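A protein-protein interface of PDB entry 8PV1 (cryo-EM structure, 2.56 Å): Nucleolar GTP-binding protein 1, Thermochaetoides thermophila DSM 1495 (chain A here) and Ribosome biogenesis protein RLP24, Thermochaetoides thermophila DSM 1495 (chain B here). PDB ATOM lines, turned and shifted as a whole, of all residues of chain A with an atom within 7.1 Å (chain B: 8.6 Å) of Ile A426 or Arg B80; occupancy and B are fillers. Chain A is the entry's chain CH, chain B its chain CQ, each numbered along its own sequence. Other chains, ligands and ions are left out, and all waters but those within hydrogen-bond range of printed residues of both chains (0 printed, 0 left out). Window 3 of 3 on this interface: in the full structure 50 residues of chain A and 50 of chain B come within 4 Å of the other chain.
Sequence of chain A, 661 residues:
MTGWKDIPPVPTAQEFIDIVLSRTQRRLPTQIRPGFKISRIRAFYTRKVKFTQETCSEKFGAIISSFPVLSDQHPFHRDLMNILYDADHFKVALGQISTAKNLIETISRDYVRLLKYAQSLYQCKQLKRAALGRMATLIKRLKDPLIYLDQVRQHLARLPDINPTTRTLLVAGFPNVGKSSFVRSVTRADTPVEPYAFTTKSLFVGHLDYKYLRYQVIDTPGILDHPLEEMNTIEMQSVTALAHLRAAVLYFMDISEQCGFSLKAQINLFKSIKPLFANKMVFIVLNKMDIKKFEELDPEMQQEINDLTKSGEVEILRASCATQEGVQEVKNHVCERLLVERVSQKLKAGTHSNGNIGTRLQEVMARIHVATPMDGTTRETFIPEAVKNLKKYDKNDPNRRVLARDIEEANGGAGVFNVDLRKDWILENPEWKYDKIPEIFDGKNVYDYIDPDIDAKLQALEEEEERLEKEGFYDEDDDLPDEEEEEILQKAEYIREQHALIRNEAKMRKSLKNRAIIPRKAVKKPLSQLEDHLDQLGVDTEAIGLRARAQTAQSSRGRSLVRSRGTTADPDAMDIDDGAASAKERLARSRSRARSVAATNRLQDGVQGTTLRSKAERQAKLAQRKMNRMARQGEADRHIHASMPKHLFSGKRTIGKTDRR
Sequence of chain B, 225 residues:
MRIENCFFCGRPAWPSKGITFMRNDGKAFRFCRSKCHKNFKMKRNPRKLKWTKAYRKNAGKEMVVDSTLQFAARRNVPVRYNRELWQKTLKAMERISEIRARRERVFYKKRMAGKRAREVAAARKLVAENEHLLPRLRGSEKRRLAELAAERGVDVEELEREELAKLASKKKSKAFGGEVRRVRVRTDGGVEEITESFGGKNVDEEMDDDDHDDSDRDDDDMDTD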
ATOM      1  N   ARG A 422      24.713 -14.854 -18.887  1.00  0.00           N
ATOM      2  CA  ARG A 422      24.379 -13.479 -19.227  1.00  0.00           C
ATOM      3  C   ARG A 422      23.294 -13.380 -20.289  1.00  0.00           C
ATOM      4  O   ARG A 422      23.013 -12.276 -20.763  1.00  0.00           O
ATOM      5  CB  ARG A 422      25.628 -12.734 -19.700  1.00  0.00           C
ATOM      6  CG  ARG A 422      26.583 -12.354 -18.586  1.00  0.00           C
ATOM      7  CD  ARG A 422      28.005 -12.350 -19.087  1.00  0.00           C
ATOM      8  NE  ARG A 422      28.949 -11.898 -18.075  1.00  0.00           N
ATOM      9  CZ  ARG A 422      29.573 -10.729 -18.107  1.00  0.00           C
ATOM     10  NH1 ARG A 422      29.350  -9.855 -19.073  1.00  0.00           N
ATOM     11  NH2 ARG A 422      30.444 -10.433 -17.148  1.00  0.00           N
ATOM     12  N   LYS A 423      22.691 -14.503 -20.679  1.00  0.00           N
ATOM     13  CA  LYS A 423      21.663 -14.482 -21.714  1.00  0.00           C
ATOM     14  C   LYS A 423      20.386 -13.811 -21.221  1.00  0.00           C
ATOM     15  O   LYS A 423      19.720 -13.093 -21.976  1.00  0.00           O
ATOM     16  CB  LYS A 423      21.377 -15.908 -22.184  1.00  0.00           C
ATOM     17  CG  LYS A 423      20.348 -16.014 -23.293  1.00  0.00           C
ATOM     18  CD  LYS A 423      20.231 -17.440 -23.796  1.00  0.00           C
ATOM     19  CE  LYS A 423      19.545 -18.324 -22.770  1.00  0.00           C
ATOM     20  NZ  LYS A 423      18.110 -17.966 -22.604  1.00  0.00           N
ATOM     21  N   ASP A 424      20.033 -14.020 -19.952  1.00  0.00           N
ATOM     22  CA  ASP A 424      18.784 -13.524 -19.393  1.00  0.00           C
ATOM     23  C   ASP A 424      18.966 -12.249 -18.579  1.00  0.00           C
ATOM     24  O   ASP A 424      18.117 -11.933 -17.739  1.00  0.00           O
ATOM     25  CB  ASP A 424      18.128 -14.607 -18.537  1.00  0.00           C
ATOM     26  CG  ASP A 424      17.534 -15.723 -19.367  1.00  0.00           C
ATOM     27  OD1 ASP A 424      17.396 -15.543 -20.594  1.00  0.00           O
ATOM     28  OD2 ASP A 424      17.211 -16.784 -18.794  1.00  0.00           O
ATOM     29  N   TRP A 425      20.054 -11.516 -18.802  1.00  0.00           N
ATOM     30  CA  TRP A 425      20.251 -10.245 -18.122  1.00  0.00           C
ATOM     31  C   TRP A 425      19.306  -9.190 -18.679  1.00  0.00           C
ATOM     32  O   TRP A 425      19.009  -9.167 -19.876  1.00  0.00           O
ATOM     33  CB  TRP A 425      21.698  -9.779 -18.268  1.00  0.00           C
ATOM     34  CG  TRP A 425      22.610 -10.295 -17.204  1.00  0.00           C
ATOM     35  CD1 TRP A 425      22.325 -11.247 -16.273  1.00  0.00           C
ATOM     36  CD2 TRP A 425      23.962  -9.890 -16.964  1.00  0.00           C
ATOM     37  NE1 TRP A 425      23.412 -11.459 -15.465  1.00  0.00           N
ATOM     38  CE2 TRP A 425      24.432 -10.638 -15.869  1.00  0.00           C
ATOM     39  CE3 TRP A 425      24.819  -8.964 -17.566  1.00  0.00           C
ATOM     40  CZ2 TRP A 425      25.721 -10.491 -15.362  1.00  0.00           C
ATOM     41  CZ3 TRP A 425      26.098  -8.822 -17.064  1.00  0.00           C
ATOM     42  CH2 TRP A 425      26.536  -9.579 -15.972  1.00  0.00           C
ATOM     43  N   ILE A 426      18.827  -8.317 -17.801  1.00  0.00           N
ATOM     44  CA  ILE A 426      17.946  -7.217 -18.169  1.00  0.00           C
ATOM     45  C   ILE A 426      18.727  -5.928 -17.973  1.00  0.00           C
ATOM     46  O   ILE A 426      18.940  -5.486 -16.837  1.00  0.00           O
ATOM     47  CB  ILE A 426      16.655  -7.215 -17.341  1.00  0.00           C
ATOM     48  CG1 ILE A 426      15.928  -8.554 -17.477  1.00  0.00           C
ATOM     49  CG2 ILE A 426      15.754  -6.071 -17.770  1.00  0.00           C
ATOM     50  CD1 ILE A 426      14.901  -8.792 -16.396  1.00  0.00           C
ATOM     51  N   LEU A 427      19.156  -5.321 -19.073  1.00  0.00           N
ATOM     52  CA  LEU A 427      19.928  -4.092 -19.035  1.00  0.00           C
ATOM     53  C   LEU A 427      19.206  -3.003 -19.816  1.00  0.00           C
ATOM     54  O   LEU A 427      18.278  -3.272 -20.583  1.00  0.00           O
ATOM     55  CB  LEU A 427      21.338  -4.303 -19.603  1.00  0.00           C
ATOM     56  CG  LEU A 427      22.172  -5.415 -18.961  1.00  0.00           C
ATOM     57  CD1 LEU A 427      23.565  -5.449 -19.557  1.00  0.00           C
ATOM     58  CD2 LEU A 427      22.241  -5.252 -17.450  1.00  0.00           C
ATOM     59  N   GLU A 428      19.635  -1.760 -19.589  1.00  0.00           N
ATOM     60  CA  GLU A 428      19.062  -0.628 -20.310  1.00  0.00           C
ATOM     61  C   GLU A 428      19.376  -0.711 -21.798  1.00  0.00           C
ATOM     62  O   GLU A 428      18.529  -0.390 -22.639  1.00  0.00           O
ATOM     63  CB  GLU A 428      19.581   0.688 -19.723  1.00  0.00           C
ATOM     64  CG  GLU A 428      19.284   0.907 -18.235  1.00  0.00           C
ATOM     65  CD  GLU A 428      20.319   0.286 -17.299  1.00  0.00           C
ATOM     66  OE1 GLU A 428      20.872  -0.787 -17.622  1.00  0.00           O
ATOM     67  OE2 GLU A 428      20.581   0.879 -16.231  1.00  0.00           O
ATOM     68  N   ASN A 429      20.587  -1.137 -22.136  1.00  0.00           N
ATOM     69  CA  ASN A 429      21.008  -1.355 -23.514  1.00  0.00           C
ATOM     70  C   ASN A 429      21.406  -2.818 -23.654  1.00  0.00           C
ATOM     71  O   ASN A 429      22.309  -3.274 -22.933  1.00  0.00           O
ATOM     72  CB  ASN A 429      22.179  -0.432 -23.867  1.00  0.00           C
ATOM     73  CG  ASN A 429      22.542  -0.466 -25.340  1.00  0.00           C
ATOM     74  OD1 ASN A 429      21.797  -0.977 -26.169  1.00  0.00           O
ATOM     75  ND2 ASN A 429      23.701   0.087 -25.668  1.00  0.00           N
ATOM     76  N   LYS A 433      25.348  -6.769 -22.680  1.00  0.00           N
ATOM     77  CA  LYS A 433      25.102  -8.018 -21.965  1.00  0.00           C
ATOM     78  C   LYS A 433      26.325  -8.922 -21.902  1.00  0.00           C
ATOM     79  O   LYS A 433      26.371  -9.816 -21.052  1.00  0.00           O
ATOM     80  CB  LYS A 433      23.932  -8.768 -22.603  1.00  0.00           C
ATOM     81  CG  LYS A 433      22.606  -8.538 -21.896  1.00  0.00           C
ATOM     82  CD  LYS A 433      21.420  -9.001 -22.725  1.00  0.00           C
ATOM     83  CE  LYS A 433      21.530 -10.470 -23.083  1.00  0.00           C
ATOM     84  NZ  LYS A 433      20.269 -10.992 -23.672  1.00  0.00           N
ATOM     85  N   ILE A 450      31.397   2.176  -7.073  1.00  0.00           N
ATOM     86  CA  ILE A 450      30.168   2.263  -7.857  1.00  0.00           C
ATOM     87  C   ILE A 450      29.070   2.884  -7.004  1.00  0.00           C
ATOM     88  O   ILE A 450      28.748   2.391  -5.917  1.00  0.00           O
ATOM     89  CB  ILE A 450      29.761   0.886  -8.390  1.00  0.00           C
ATOM     90  CG1 ILE A 450      30.673   0.486  -9.545  1.00  0.00           C
ATOM     91  CG2 ILE A 450      28.310   0.889  -8.851  1.00  0.00           C
ATOM     92  CD1 ILE A 450      30.493   1.340 -10.768  1.00  0.00           C
ATOM     93  N   VAL B  77      23.719  -2.685  -1.491  1.00  0.00           N
ATOM     94  CA  VAL B  77      22.604  -2.609  -2.431  1.00  0.00           C
ATOM     95  C   VAL B  77      23.185  -2.561  -3.839  1.00  0.00           C
ATOM     96  O   VAL B  77      23.790  -1.551  -4.221  1.00  0.00           O
ATOM     97  CB  VAL B  77      21.707  -1.395  -2.148  1.00  0.00           C
ATOM     98  CG1 VAL B  77      20.542  -1.361  -3.122  1.00  0.00           C
ATOM     99  CG2 VAL B  77      21.207  -1.434  -0.719  1.00  0.00           C
ATOM    100  N   PRO B  78      23.046  -3.626  -4.627  1.00  0.00           N
ATOM    101  CA  PRO B  78      23.684  -3.656  -5.948  1.00  0.00           C
ATOM    102  C   PRO B  78      23.025  -2.706  -6.935  1.00  0.00           C
ATOM    103  O   PRO B  78      21.836  -2.394  -6.842  1.00  0.00           O
ATOM    104  CB  PRO B  78      23.518  -5.115  -6.386  1.00  0.00           C
ATOM    105  CG  PRO B  78      22.338  -5.600  -5.623  1.00  0.00           C
ATOM    106  CD  PRO B  78      22.396  -4.905  -4.300  1.00  0.00           C
ATOM    107  N   VAL B  79      23.824  -2.248  -7.893  1.00  0.00           N
ATOM    108  CA  VAL B  79      23.386  -1.364  -8.964  1.00  0.00           C
ATOM    109  C   VAL B  79      23.408  -2.153 -10.265  1.00  0.00           C
ATOM    110  O   VAL B  79      24.337  -2.933 -10.508  1.00  0.00           O
ATOM    111  CB  VAL B  79      24.285  -0.111  -9.045  1.00  0.00           C
ATOM    112  CG1 VAL B  79      23.877   0.796 -10.199  1.00  0.00           C
ATOM    113  CG2 VAL B  79      24.240   0.650  -7.734  1.00  0.00           C
ATOM    114  N   ARG B  80      22.362  -1.986 -11.076  1.00  0.00           N
ATOM    115  CA  ARG B  80      22.312  -2.613 -12.391  1.00  0.00           C
ATOM    116  C   ARG B  80      23.457  -2.105 -13.261  1.00  0.00           C
ATOM    117  O   ARG B  80      23.824  -0.928 -13.204  1.00  0.00           O
ATOM    118  CB  ARG B  80      20.967  -2.322 -13.056  1.00  0.00           C
ATOM    119  CG  ARG B  80      20.741  -3.034 -14.377  1.00  0.00           C
ATOM    120  CD  ARG B  80      19.302  -2.887 -14.839  1.00  0.00           C
ATOM    121  NE  ARG B  80      18.353  -3.309 -13.816  1.00  0.00           N
ATOM    122  CZ  ARG B  80      17.932  -4.555 -13.650  1.00  0.00           C
ATOM    123  NH1 ARG B  80      18.369  -5.540 -14.416  1.00  0.00           N
ATOM    124  NH2 ARG B  80      17.055  -4.820 -12.688  1.00  0.00           N
ATOM    125  N   TYR B  81      24.033  -3.005 -14.056  1.00  0.00           N
ATOM    126  CA  TYR B  81      25.259  -2.694 -14.780  1.00  0.00           C
ATOM    127  C   TYR B  81      25.003  -1.679 -15.889  1.00  0.00           C
ATOM    128  O   TYR B  81      24.048  -1.807 -16.661  1.00  0.00           O
ATOM    129  CB  TYR B  81      25.876  -3.963 -15.364  1.00  0.00           C
ATOM    130  CG  TYR B  81      26.962  -3.667 -16.370  1.00  0.00           C
ATOM    131  CD1 TYR B  81      28.163  -3.097 -15.969  1.00  0.00           C
ATOM    132  CD2 TYR B  81      26.780  -3.929 -17.720  1.00  0.00           C
ATOM    133  CE1 TYR B  81      29.153  -2.809 -16.879  1.00  0.00           C
ATOM    134  CE2 TYR B  81      27.766  -3.644 -18.637  1.00  0.00           C
ATOM    135  CZ  TYR B  81      28.951  -3.086 -18.211  1.00  0.00           C
ATOM    136  OH  TYR B  81      29.935  -2.804 -19.126  1.00  0.00           O
ATOM    137  N   ASN B  82      25.872  -0.671 -15.967  1.00  0.00           N
ATOM    138  CA  ASN B  82      25.767   0.393 -16.956  1.00  0.00           C
ATOM    139  C   ASN B  82      27.178   0.766 -17.387  1.00  0.00           C
ATOM    140  O   ASN B  82      28.014   1.113 -16.543  1.00  0.00           O
ATOM    141  CB  ASN B  82      25.022   1.601 -16.379  1.00  0.00           C
ATOM    142  CG  ASN B  82      24.553   2.575 -17.443  1.00  0.00           C
ATOM    143  OD1 ASN B  82      25.272   2.889 -18.388  1.00  0.00           O
ATOM    144  ND2 ASN B  82      23.326   3.052 -17.294  1.00  0.00           N
ATOM    145  N   ARG B  83      27.434   0.696 -18.697  1.00  0.00           N
ATOM    146  CA  ARG B  83      28.787   0.891 -19.212  1.00  0.00           C
ATOM    147  C   ARG B  83      29.298   2.303 -18.943  1.00  0.00           C
ATOM    148  O   ARG B  83      30.445   2.482 -18.513  1.00  0.00           O
ATOM    149  CB  ARG B  83      28.822   0.575 -20.708  1.00  0.00           C
ATOM    150  CG  ARG B  83      30.202   0.656 -21.332  1.00  0.00           C
ATOM    151  CD  ARG B  83      30.159   0.382 -22.825  1.00  0.00           C
ATOM    152  NE  ARG B  83      29.760  -0.987 -23.126  1.00  0.00           N
ATOM    153  CZ  ARG B  83      29.584  -1.460 -24.352  1.00  0.00           C
ATOM    154  NH1 ARG B  83      29.774  -0.702 -25.419  1.00  0.00           N
ATOM    155  NH2 ARG B  83      29.205  -2.724 -24.513  1.00  0.00           N
ATOM    156  N   LEU B  85      28.284   4.308 -16.574  1.00  0.00           N
ATOM    157  CA  LEU B  85      28.456   4.460 -15.133  1.00  0.00           C
ATOM    158  C   LEU B  85      29.779   3.863 -14.669  1.00  0.00           C
ATOM    159  O   LEU B  85      30.499   4.483 -13.879  1.00  0.00           O
ATOM    160  CB  LEU B  85      27.281   3.823 -14.392  1.00  0.00           C
ATOM    161  CG  LEU B  85      27.383   3.790 -12.866  1.00  0.00           C
ATOM    162  CD1 LEU B  85      27.403   5.203 -12.307  1.00  0.00           C
ATOM    163  CD2 LEU B  85      26.237   2.992 -12.268  1.00  0.00           C
ATOM    164  N   TRP B  86      30.137   2.680 -15.179  1.00  0.00           N
ATOM    165  CA  TRP B  86      31.439   2.097 -14.848  1.00  0.00           C
ATOM    166  C   TRP B  86      32.604   2.926 -15.390  1.00  0.00           C
ATOM    167  O   TRP B  86      33.626   3.080 -14.706  1.00  0.00           O
ATOM    168  CB  TRP B  86      31.507   0.647 -15.331  1.00  0.00           C
ATOM    169  CG  TRP B  86      31.235  -0.361 -14.241  1.00  0.00           C
ATOM    170  CD1 TRP B  86      32.165  -1.119 -13.591  1.00  0.00           C
ATOM    171  CD2 TRP B  86      29.980  -0.652 -13.613  1.00  0.00           C
ATOM    172  NE1 TRP B  86      31.565  -1.899 -12.637  1.00  0.00           N
ATOM    173  CE2 TRP B  86      30.223  -1.627 -12.626  1.00  0.00           C
ATOM    174  CE3 TRP B  86      28.674  -0.196 -13.798  1.00  0.00           C
ATOM    175  CZ2 TRP B  86      29.210  -2.152 -11.832  1.00  0.00           C
ATOM    176  CZ3 TRP B  86      27.670  -0.719 -13.010  1.00  0.00           C
ATOM    177  CH2 TRP B  86      27.943  -1.688 -12.040  1.00  0.00           C
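The guanidinium group of Arg B80 sits at hydrogen-bond distance from the backbone carbonyl oxygen of Ile A426, at 2.5 Å.
The side-chain carboxylate (OE1) of Glu A428 lies close to the backbone carbonyl oxygen (O) of Tyr B81, at 3.5 Å.
Among the printed residues, merely in contact across the chains: Ile A450 with Trp B86 (3.5 Å), Glu A428 with Asn B82 (3.7 Å), Glu A428 with Arg B80 (3.8 Å) and Leu A427 with Tyr B81 (3.97 Å).
Of chain B, only Arg B80 (2.5 Å) comes within 4 Å of Ile A426.
Arg B80 touches two residues of chain A.
Of the printed residues of chain B, Leu A427 touches Tyr B81.
Printed residues of chain B within 4 Å of Glu A428: Arg B80, Tyr B81 and Asn B82.
Of the printed residues of chain A, Trp B86 touches Ile A450.
Of the printed residues of chain B, Ile A450 touches Trp B86.
Of the printed residues of chain A, Tyr B81 touches Leu A427 (3.97 Å) and Glu A428 (3.5 Å).
The nearest residue of chain B that does not touch Ile A426 is Tyr B81 (6.3 Å).
Of the 9 printed residues of chain B, 4 touch a printed residue of chain A.
Hydrophobic or aromatic side chains of chain B that line the printed part of chain A: Trp B86.
Of the 10 printed residues of chain A, 4 touch a printed residue of chain B.
Hydrophobic or aromatic side chains of chain A that line the printed part of chain B: Ile A426, Leu A427 and Ile A450.
Among the printed residues, 6 pairs touch across the chains.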
